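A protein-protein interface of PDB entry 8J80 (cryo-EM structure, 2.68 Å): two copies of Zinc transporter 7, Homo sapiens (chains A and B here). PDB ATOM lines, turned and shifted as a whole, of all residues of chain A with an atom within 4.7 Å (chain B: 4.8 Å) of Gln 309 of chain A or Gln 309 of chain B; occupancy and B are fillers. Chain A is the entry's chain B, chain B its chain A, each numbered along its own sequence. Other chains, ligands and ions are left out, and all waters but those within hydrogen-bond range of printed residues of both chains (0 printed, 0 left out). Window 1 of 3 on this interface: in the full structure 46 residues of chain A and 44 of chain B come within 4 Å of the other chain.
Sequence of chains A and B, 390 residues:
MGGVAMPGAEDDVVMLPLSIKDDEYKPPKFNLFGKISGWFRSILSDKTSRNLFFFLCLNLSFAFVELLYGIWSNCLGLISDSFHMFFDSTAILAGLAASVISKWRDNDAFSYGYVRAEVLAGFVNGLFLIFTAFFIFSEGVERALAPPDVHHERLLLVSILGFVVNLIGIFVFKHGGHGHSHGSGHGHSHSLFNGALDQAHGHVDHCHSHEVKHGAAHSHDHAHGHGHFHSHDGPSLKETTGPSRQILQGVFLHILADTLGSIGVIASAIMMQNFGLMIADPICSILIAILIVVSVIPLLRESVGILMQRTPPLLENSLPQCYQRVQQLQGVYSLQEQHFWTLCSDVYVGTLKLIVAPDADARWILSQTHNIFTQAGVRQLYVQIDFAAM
Of the 12 printed residues of chain B, 6 touch a printed residue of chain A.
Printed residues of chain B that touch a printed residue of chain A: Tyr 112, Arg 116, Leu 307, Met 308, Gln 309 and Trp 341.
Of the 12 printed residues of chain A, 6 touch a printed residue of chain B.
Hydrophobic or aromatic side chains of chain A within 4 Å of the printed part of chain B: Tyr 112, Leu 307, Met 308 and Trp 341.
NH1 of Arg 116 of chain B lies within hydrogen-bond range of O of Leu 307 of chain A (3.1 Å).
The side-chain amide oxygen of Gln 309 of chain A sits at hydrogen-bond distance from the guanidinium group of Arg 116 of chain B, at 3.4 Å.
The backbone carbonyl oxygen (O) of Leu 307 of chain B is in hydrogen-bond range of the guanidinium group (NH1) of Arg 116 of chain A (3.0 Å).
OE1 of Gln 309 of chain B sits at hydrogen-bond distance from NH1 of Arg 116 of chain A (3.4 Å).
NE2 of Gln 309 of chain B sits close to NE2 of Gln 309 of chain A, at 3.5 Å.
OE1 of Gln 309 of chain B sits at hydrogen-bond distance from NH2 of Arg 116 of chain B, at 3.0 Å.
The guanidinium group (NE) of Arg 116 of chain B sits at hydrogen-bond distance from the backbone carbonyl oxygen (O) of Leu 343 of chain B (2.9 Å).
The guanidinium group of Arg 116 of chain A lies within hydrogen-bond range of the side-chain amide oxygen of Gln 309 of chain A (2.8 Å).
The guanidinium group (NE) of Arg 116 of chain A is in hydrogen-bond range of the backbone carbonyl oxygen (O) of Leu 343 of chain A, at 2.9 Å.
O of Ile 306 of chain A lies close to OE1 of Gln 309 of chain A, at 3.4 Å.
Of the printed residues of chain B, Met 308 of chain A touches Arg 116 (3.7 Å).
Printed residues of chain B within 4 Å of Gln 309 of chain A: Tyr 112 (3.95 Å), Arg 116 (3.4 Å), Gln 309 (3.5 Å) and Trp 341 (3.5 Å).
Of the printed residues of chain A, Tyr 112 of chain B touches Gln 309 (3.95 Å) and Trp 341 (3.96 Å).
Of the printed residues of chain A, Arg 116 of chain B touches Arg 116 (3.9 Å), Leu 307 (3.1 Å), Met 308 (3.7 Å) and Gln 309 (3.4 Å).
Gln 309 of chain B touches just these residues of chain A: Tyr 112, Arg 116, Gln 309 and Trp 341.
Thr 311 of chain B touches none of the printed residues of chain A.
The nearest residue of chain B that does not touch Gln 309 of chain A is Leu 343 of chain B (4.3 Å).
The nearest residue of chain A that does not touch Gln 309 of chain B is Leu 343 of chain A (4.2 Å).
Tyr 112 of chain A touches Gln 309 of chain B, and with the chains exchanged Gln 309 of chain A touches Tyr 112 of chain B.
Arg 116 of chain A touches Leu 307 of chain B, and with the chains exchanged Leu 307 of chain A touches Arg 116 of chain B.
Leu 307 of chain B touches its own counterpart, Leu 307 of chain A.
Trp 341 of chain A touches its own counterpart, Trp 341 of chain B.
Positions printed for both chains: 112, 116, 305, 306, 307, 308, 309, 310, 311, 340, 341 and 343.
CB of Gln 309 of chain B touches CD2 of Tyr 112 of chain A, at 3.9 Å.
Arg 116 of chain B touches Arg 116 of chain A (NH1 to NH1, 3.9 Å).
SD of Met 308 of chain B touches CB of Arg 116 of chain A, 3.7 Å away.
O of Leu 307 of chain B touches CD2 of Leu 307 of chain A (3.8 Å).
Met 308 of chain A touches Arg 116 of chain B (CA to CB, 3.7 Å).
Tyr 112 of chain B touches Gln 309 of chain A.
NE2 of Gln 309 of chain A touches CH2 of Trp 341 of chain B, at 3.5 Å.
Tyr 112 of chain B touches Trp 341 of chain A (CE2 to CD1, 3.96 Å).
NE2 of Gln 309 of chain B touches CH2 of Trp 341 of chain A (3.3 Å).
Trp 341 of chain A touches Trp 341 of chain B.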
ATOM      1  N   TYR A 112      19.268   4.402  -8.295  1.00  0.00           N
ATOM      2  CA  TYR A 112      19.737   3.794  -9.529  1.00  0.00           C
ATOM      3  C   TYR A 112      19.308   4.579 -10.759  1.00  0.00           C
ATOM      4  O   TYR A 112      19.608   4.165 -11.880  1.00  0.00           O
ATOM      5  CB  TYR A 112      19.238   2.352  -9.625  1.00  0.00           C
ATOM      6  CG  TYR A 112      20.027   1.376  -8.786  1.00  0.00           C
ATOM      7  CD1 TYR A 112      21.340   1.073  -9.098  1.00  0.00           C
ATOM      8  CD2 TYR A 112      19.457   0.765  -7.683  1.00  0.00           C
ATOM      9  CE1 TYR A 112      22.062   0.189  -8.344  1.00  0.00           C
ATOM     10  CE2 TYR A 112      20.175  -0.118  -6.916  1.00  0.00           C
ATOM     11  CZ  TYR A 112      21.480  -0.407  -7.255  1.00  0.00           C
ATOM     12  OH  TYR A 112      22.212  -1.290  -6.494  1.00  0.00           O
ATOM     13  N   ARG A 116      15.232   1.798 -15.273  1.00  0.00           N
ATOM     14  CA  ARG A 116      14.317   0.681 -15.446  1.00  0.00           C
ATOM     15  C   ARG A 116      13.112   1.042 -16.298  1.00  0.00           C
ATOM     16  O   ARG A 116      12.445   0.137 -16.810  1.00  0.00           O
ATOM     17  CB  ARG A 116      13.858   0.162 -14.085  1.00  0.00           C
ATOM     18  CG  ARG A 116      14.837  -0.789 -13.437  1.00  0.00           C
ATOM     19  CD  ARG A 116      14.570  -2.214 -13.852  1.00  0.00           C
ATOM     20  NE  ARG A 116      15.576  -3.125 -13.327  1.00  0.00           N
ATOM     21  CZ  ARG A 116      15.364  -3.994 -12.351  1.00  0.00           C
ATOM     22  NH1 ARG A 116      14.187  -4.100 -11.762  1.00  0.00           N
ATOM     23  NH2 ARG A 116      16.361  -4.775 -11.954  1.00  0.00           N
ATOM     24  N   GLY A 305      12.347 -11.732 -16.796  1.00  0.00           N
ATOM     25  CA  GLY A 305      13.630 -12.132 -16.250  1.00  0.00           C
ATOM     26  C   GLY A 305      14.383 -10.984 -15.607  1.00  0.00           C
ATOM     27  O   GLY A 305      14.950 -11.135 -14.526  1.00  0.00           O
ATOM     28  N   ILE A 306      14.390  -9.820 -16.253  1.00  0.00           N
ATOM     29  CA  ILE A 306      15.063  -8.671 -15.646  1.00  0.00           C
ATOM     30  C   ILE A 306      14.348  -8.231 -14.369  1.00  0.00           C
ATOM     31  O   ILE A 306      14.987  -7.955 -13.349  1.00  0.00           O
ATOM     32  CB  ILE A 306      15.186  -7.520 -16.657  1.00  0.00           C
ATOM     33  CG1 ILE A 306      16.157  -7.904 -17.770  1.00  0.00           C
ATOM     34  CG2 ILE A 306      15.641  -6.246 -15.964  1.00  0.00           C
ATOM     35  CD1 ILE A 306      15.988  -7.116 -19.019  1.00  0.00           C
ATOM     36  N   LEU A 307      13.021  -8.178 -14.394  1.00  0.00           N
ATOM     37  CA  LEU A 307      12.255  -7.689 -13.255  1.00  0.00           C
ATOM     38  C   LEU A 307      12.156  -8.695 -12.116  1.00  0.00           C
ATOM     39  O   LEU A 307      11.732  -8.317 -11.020  1.00  0.00           O
ATOM     40  CB  LEU A 307      10.850  -7.290 -13.701  1.00  0.00           C
ATOM     41  CG  LEU A 307      10.762  -6.069 -14.614  1.00  0.00           C
ATOM     42  CD1 LEU A 307       9.359  -5.906 -15.164  1.00  0.00           C
ATOM     43  CD2 LEU A 307      11.208  -4.820 -13.881  1.00  0.00           C
ATOM     44  N   MET A 308      12.523  -9.952 -12.339  1.00  0.00           N
ATOM     45  CA  MET A 308      12.549 -10.955 -11.287  1.00  0.00           C
ATOM     46  C   MET A 308      13.867 -10.970 -10.530  1.00  0.00           C
ATOM     47  O   MET A 308      14.066 -11.847  -9.687  1.00  0.00           O
ATOM     48  CB  MET A 308      12.271 -12.348 -11.861  1.00  0.00           C
ATOM     49  CG  MET A 308      10.815 -12.602 -12.220  1.00  0.00           C
ATOM     50  SD  MET A 308       9.799 -13.275 -10.897  1.00  0.00           S
ATOM     51  CE  MET A 308      10.921 -14.434 -10.143  1.00  0.00           C
ATOM     52  N   GLN A 309      14.757 -10.012 -10.812  1.00  0.00           N
ATOM     53  CA  GLN A 309      16.110  -9.943 -10.249  1.00  0.00           C
ATOM     54  C   GLN A 309      16.910 -11.201 -10.558  1.00  0.00           C
ATOM     55  O   GLN A 309      17.665 -11.696  -9.726  1.00  0.00           O
ATOM     56  CB  GLN A 309      16.090  -9.666  -8.743  1.00  0.00           C
ATOM     57  CG  GLN A 309      15.475  -8.340  -8.363  1.00  0.00           C
ATOM     58  CD  GLN A 309      16.085  -7.172  -9.103  1.00  0.00           C
ATOM     59  OE1 GLN A 309      15.618  -6.792 -10.170  1.00  0.00           O
ATOM     60  NE2 GLN A 309      17.117  -6.581  -8.529  1.00  0.00           N
ATOM     61  N   ARG A 310      16.755 -11.704 -11.776  1.00  0.00           N
ATOM     62  CA  ARG A 310      17.440 -12.904 -12.223  1.00  0.00           C
ATOM     63  C   ARG A 310      18.889 -12.592 -12.585  1.00  0.00           C
ATOM     64  O   ARG A 310      19.223 -11.473 -12.977  1.00  0.00           O
ATOM     65  CB  ARG A 310      16.698 -13.498 -13.420  1.00  0.00           C
ATOM     66  CG  ARG A 310      17.203 -14.812 -13.945  1.00  0.00           C
ATOM     67  CD  ARG A 310      17.143 -14.852 -15.446  1.00  0.00           C
ATOM     68  NE  ARG A 310      17.370 -16.197 -15.956  1.00  0.00           N
ATOM     69  CZ  ARG A 310      18.564 -16.732 -16.161  1.00  0.00           C
ATOM     70  NH1 ARG A 310      19.675 -16.053 -15.933  1.00  0.00           N
ATOM     71  NH2 ARG A 310      18.645 -17.982 -16.603  1.00  0.00           N
ATOM     72  N   THR A 311      19.748 -13.591 -12.431  1.00  0.00           N
ATOM     73  CA  THR A 311      21.119 -13.483 -12.900  1.00  0.00           C
ATOM     74  C   THR A 311      21.125 -13.198 -14.397  1.00  0.00           C
ATOM     75  O   THR A 311      20.407 -13.871 -15.147  1.00  0.00           O
ATOM     76  CB  THR A 311      21.887 -14.771 -12.603  1.00  0.00           C
ATOM     77  OG1 THR A 311      22.026 -14.929 -11.190  1.00  0.00           O
ATOM     78  CG2 THR A 311      23.263 -14.736 -13.218  1.00  0.00           C
ATOM     79  N   PHE A 340      23.857 -11.379  -8.609  1.00  0.00           N
ATOM     80  CA  PHE A 340      24.106 -10.591  -9.807  1.00  0.00           C
ATOM     81  C   PHE A 340      22.786 -10.400 -10.527  1.00  0.00           C
ATOM     82  O   PHE A 340      22.021 -11.352 -10.676  1.00  0.00           O
ATOM     83  CB  PHE A 340      25.138 -11.269 -10.716  1.00  0.00           C
ATOM     84  CG  PHE A 340      26.487 -11.395 -10.087  1.00  0.00           C
ATOM     85  CD1 PHE A 340      26.785 -12.467  -9.270  1.00  0.00           C
ATOM     86  CD2 PHE A 340      27.452 -10.435 -10.297  1.00  0.00           C
ATOM     87  CE1 PHE A 340      28.012 -12.572  -8.681  1.00  0.00           C
ATOM     88  CE2 PHE A 340      28.678 -10.534  -9.704  1.00  0.00           C
ATOM     89  CZ  PHE A 340      28.960 -11.608  -8.898  1.00  0.00           C
ATOM     90  N   TRP A 341      22.500  -9.169 -10.933  1.00  0.00           N
ATOM     91  CA  TRP A 341      21.244  -8.899 -11.614  1.00  0.00           C
ATOM     92  C   TRP A 341      21.429  -7.801 -12.644  1.00  0.00           C
ATOM     93  O   TRP A 341      22.351  -6.990 -12.573  1.00  0.00           O
ATOM     94  CB  TRP A 341      20.116  -8.535 -10.636  1.00  0.00           C
ATOM     95  CG  TRP A 341      20.443  -7.489  -9.600  1.00  0.00           C
ATOM     96  CD1 TRP A 341      21.054  -7.691  -8.402  1.00  0.00           C
ATOM     97  CD2 TRP A 341      20.150  -6.086  -9.666  1.00  0.00           C
ATOM     98  NE1 TRP A 341      21.162  -6.511  -7.723  1.00  0.00           N
ATOM     99  CE2 TRP A 341      20.616  -5.509  -8.476  1.00  0.00           C
ATOM    100  CE3 TRP A 341      19.538  -5.267 -10.618  1.00  0.00           C
ATOM    101  CZ2 TRP A 341      20.490  -4.150  -8.207  1.00  0.00           C
ATOM    102  CZ3 TRP A 341      19.412  -3.923 -10.351  1.00  0.00           C
ATOM    103  CH2 TRP A 341      19.889  -3.374  -9.157  1.00  0.00           C
ATOM    104  N   LEU A 343      20.426  -4.417 -14.118  1.00  0.00           N
ATOM    105  CA  LEU A 343      19.748  -3.162 -13.829  1.00  0.00           C
ATOM    106  C   LEU A 343      19.031  -2.650 -15.068  1.00  0.00           C
ATOM    107  O   LEU A 343      17.809  -2.483 -15.075  1.00  0.00           O
ATOM    108  CB  LEU A 343      20.752  -2.130 -13.317  1.00  0.00           C
ATOM    109  CG  LEU A 343      20.199  -0.737 -13.044  1.00  0.00           C
ATOM    110  CD1 LEU A 343      19.171  -0.780 -11.924  1.00  0.00           C
ATOM    111  CD2 LEU A 343      21.320   0.220 -12.720  1.00  0.00           C
ATOM    112  N   TYR B 112      17.859 -14.491  -5.777  1.00  0.00           N
ATOM    113  CA  TYR B 112      16.980 -13.930  -4.773  1.00  0.00           C
ATOM    114  C   TYR B 112      15.713 -14.751  -4.602  1.00  0.00           C
ATOM    115  O   TYR B 112      14.798 -14.323  -3.894  1.00  0.00           O
ATOM    116  CB  TYR B 112      16.640 -12.487  -5.135  1.00  0.00           C
ATOM    117  CG  TYR B 112      17.755 -11.510  -4.852  1.00  0.00           C
ATOM    118  CD1 TYR B 112      18.065 -11.148  -3.555  1.00  0.00           C
ATOM    119  CD2 TYR B 112      18.494 -10.949  -5.883  1.00  0.00           C
ATOM    120  CE1 TYR B 112      19.070 -10.260  -3.287  1.00  0.00           C
ATOM    121  CE2 TYR B 112      19.505 -10.058  -5.625  1.00  0.00           C
ATOM    122  CZ  TYR B 112      19.790  -9.715  -4.318  1.00  0.00           C
ATOM    123  OH  TYR B 112      20.801  -8.829  -4.034  1.00  0.00           O
ATOM    124  N   ARG B 116       9.824 -12.151  -6.447  1.00  0.00           N
ATOM    125  CA  ARG B 116       9.346 -11.028  -7.240  1.00  0.00           C
ATOM    126  C   ARG B 116       8.044 -11.347  -7.955  1.00  0.00           C
ATOM    127  O   ARG B 116       7.338 -10.425  -8.370  1.00  0.00           O
ATOM    128  CB  ARG B 116      10.419 -10.608  -8.241  1.00  0.00           C
ATOM    129  CG  ARG B 116      11.422  -9.626  -7.682  1.00  0.00           C
ATOM    130  CD  ARG B 116      10.894  -8.219  -7.777  1.00  0.00           C
ATOM    131  NE  ARG B 116      11.698  -7.257  -7.037  1.00  0.00           N
ATOM    132  CZ  ARG B 116      12.434  -6.314  -7.600  1.00  0.00           C
ATOM    133  NH1 ARG B 116      12.542  -6.214  -8.913  1.00  0.00           N
ATOM    134  NH2 ARG B 116      13.074  -5.445  -6.827  1.00  0.00           N
ATOM    135  N   GLY B 305       7.121   1.383  -8.073  1.00  0.00           N
ATOM    136  CA  GLY B 305       8.271   1.794  -7.287  1.00  0.00           C
ATOM    137  C   GLY B 305       9.200   0.643  -6.955  1.00  0.00           C
ATOM    138  O   GLY B 305      10.420   0.784  -7.017  1.00  0.00           O
ATOM    139  N   ILE B 306       8.637  -0.511  -6.599  1.00  0.00           N
ATOM    140  CA  ILE B 306       9.466  -1.675  -6.303  1.00  0.00           C
ATOM    141  C   ILE B 306      10.204  -2.140  -7.551  1.00  0.00           C
ATOM    142  O   ILE B 306      11.413  -2.393  -7.519  1.00  0.00           O
ATOM    143  CB  ILE B 306       8.612  -2.800  -5.696  1.00  0.00           C
ATOM    144  CG1 ILE B 306       8.122  -2.396  -4.305  1.00  0.00           C
ATOM    145  CG2 ILE B 306       9.392  -4.104  -5.642  1.00  0.00           C
ATOM    146  CD1 ILE B 306       7.120  -3.346  -3.715  1.00  0.00           C
ATOM    147  N   LEU B 307       9.497  -2.236  -8.677  1.00  0.00           N
ATOM    148  CA  LEU B 307      10.132  -2.721  -9.897  1.00  0.00           C
ATOM    149  C   LEU B 307      11.100  -1.715 -10.505  1.00  0.00           C
ATOM    150  O   LEU B 307      11.947  -2.103 -11.310  1.00  0.00           O
ATOM    151  CB  LEU B 307       9.067  -3.106 -10.919  1.00  0.00           C
ATOM    152  CG  LEU B 307       8.228  -4.313 -10.516  1.00  0.00           C
ATOM    153  CD1 LEU B 307       7.119  -4.561 -11.517  1.00  0.00           C
ATOM    154  CD2 LEU B 307       9.104  -5.542 -10.352  1.00  0.00           C
ATOM    155  N   MET B 308      11.008  -0.444 -10.135  1.00  0.00           N
ATOM    156  CA  MET B 308      11.911   0.576 -10.641  1.00  0.00           C
ATOM    157  C   MET B 308      13.163   0.727  -9.791  1.00  0.00           C
ATOM    158  O   MET B 308      13.924   1.670 -10.006  1.00  0.00           O
ATOM    159  CB  MET B 308      11.187   1.919 -10.746  1.00  0.00           C
ATOM    160  CG  MET B 308      10.382   2.086 -12.022  1.00  0.00           C
ATOM    161  SD  MET B 308      11.298   2.796 -13.394  1.00  0.00           S
ATOM    162  CE  MET B 308      11.723   4.394 -12.723  1.00  0.00           C
ATOM    163  N   GLN B 309      13.376  -0.181  -8.835  1.00  0.00           N
ATOM    164  CA  GLN B 309      14.539  -0.217  -7.948  1.00  0.00           C
ATOM    165  C   GLN B 309      14.613   1.006  -7.046  1.00  0.00           C
ATOM    166  O   GLN B 309      15.694   1.405  -6.617  1.00  0.00           O
ATOM    167  CB  GLN B 309      15.845  -0.391  -8.731  1.00  0.00           C
ATOM    168  CG  GLN B 309      15.921  -1.706  -9.457  1.00  0.00           C
ATOM    169  CD  GLN B 309      15.811  -2.882  -8.522  1.00  0.00           C
ATOM    170  OE1 GLN B 309      14.775  -3.530  -8.450  1.00  0.00           O
ATOM    171  NE2 GLN B 309      16.885  -3.177  -7.815  1.00  0.00           N
ATOM    172  N   ARG B 310      13.459   1.578  -6.736  1.00  0.00           N
ATOM    173  CA  ARG B 310      13.355   2.763  -5.910  1.00  0.00           C
ATOM    174  C   ARG B 310      13.682   2.433  -4.454  1.00  0.00           C
ATOM    175  O   ARG B 310      13.587   1.288  -4.013  1.00  0.00           O
ATOM    176  CB  ARG B 310      11.947   3.339  -6.040  1.00  0.00           C
ATOM    177  CG  ARG B 310      11.681   4.661  -5.410  1.00  0.00           C
ATOM    178  CD  ARG B 310      10.217   4.785  -5.102  1.00  0.00           C
ATOM    179  NE  ARG B 310       9.881   6.070  -4.510  1.00  0.00           N
ATOM    180  CZ  ARG B 310      10.108   6.399  -3.247  1.00  0.00           C
ATOM    181  NH1 ARG B 310      10.686   5.558  -2.407  1.00  0.00           N
ATOM    182  NH2 ARG B 310       9.742   7.600  -2.815  1.00  0.00           N
ATOM    183  N   THR B 311      14.095   3.456  -3.716  1.00  0.00           N
ATOM    184  CA  THR B 311      14.267   3.325  -2.281  1.00  0.00           C
ATOM    185  C   THR B 311      12.926   2.984  -1.637  1.00  0.00           C
ATOM    186  O   THR B 311      11.901   3.570  -2.000  1.00  0.00           O
ATOM    187  CB  THR B 311      14.826   4.625  -1.692  1.00  0.00           C
ATOM    188  OG1 THR B 311      16.061   4.948  -2.331  1.00  0.00           O
ATOM    189  CG2 THR B 311      15.065   4.504  -0.202  1.00  0.00           C
ATOM    190  N   PHE B 340      19.494   1.324  -1.823  1.00  0.00           N
ATOM    191  CA  PHE B 340      18.535   0.520  -1.082  1.00  0.00           C
ATOM    192  C   PHE B 340      17.315   0.284  -1.954  1.00  0.00           C
ATOM    193  O   PHE B 340      16.822   1.204  -2.604  1.00  0.00           O
ATOM    194  CB  PHE B 340      18.150   1.193   0.243  1.00  0.00           C
ATOM    195  CG  PHE B 340      19.305   1.365   1.178  1.00  0.00           C
ATOM    196  CD1 PHE B 340      20.117   2.482   1.101  1.00  0.00           C
ATOM    197  CD2 PHE B 340      19.595   0.400   2.123  1.00  0.00           C
ATOM    198  CE1 PHE B 340      21.184   2.630   1.942  1.00  0.00           C
ATOM    199  CE2 PHE B 340      20.661   0.546   2.970  1.00  0.00           C
ATOM    200  CZ  PHE B 340      21.455   1.663   2.882  1.00  0.00           C
ATOM    201  N   TRP B 341      16.849  -0.960  -1.984  1.00  0.00           N
ATOM    202  CA  TRP B 341      15.684  -1.301  -2.784  1.00  0.00           C
ATOM    203  C   TRP B 341      14.874  -2.380  -2.082  1.00  0.00           C
ATOM    204  O   TRP B 341      15.314  -2.996  -1.114  1.00  0.00           O
ATOM    205  CB  TRP B 341      16.066  -1.742  -4.210  1.00  0.00           C
ATOM    206  CG  TRP B 341      17.198  -2.740  -4.335  1.00  0.00           C
ATOM    207  CD1 TRP B 341      18.530  -2.475  -4.263  1.00  0.00           C
ATOM    208  CD2 TRP B 341      17.086  -4.146  -4.597  1.00  0.00           C
ATOM    209  NE1 TRP B 341      19.251  -3.620  -4.448  1.00  0.00           N
ATOM    210  CE2 TRP B 341      18.392  -4.662  -4.657  1.00  0.00           C
ATOM    211  CE3 TRP B 341      16.008  -5.016  -4.788  1.00  0.00           C
ATOM    212  CZ2 TRP B 341      18.652  -6.009  -4.899  1.00  0.00           C
ATOM    213  CZ3 TRP B 341      16.266  -6.347  -5.024  1.00  0.00           C
ATOM    214  CH2 TRP B 341      17.577  -6.834  -5.077  1.00  0.00           C
ATOM    215  N   LEU B 343      13.091  -5.972  -2.313  1.00  0.00           N
ATOM    216  CA  LEU B 343      13.059  -7.243  -3.028  1.00  0.00           C
ATOM    217  C   LEU B 343      11.627  -7.747  -3.169  1.00  0.00           C
ATOM    218  O   LEU B 343      11.092  -7.843  -4.276  1.00  0.00           O
ATOM    219  CB  LEU B 343      13.921  -8.268  -2.294  1.00  0.00           C
ATOM    220  CG  LEU B 343      14.030  -9.640  -2.946  1.00  0.00           C
ATOM    221  CD1 LEU B 343      14.758  -9.530  -4.273  1.00  0.00           C
ATOM    222  CD2 LEU B 343      14.714 -10.619  -2.021  1.00  0.00           C
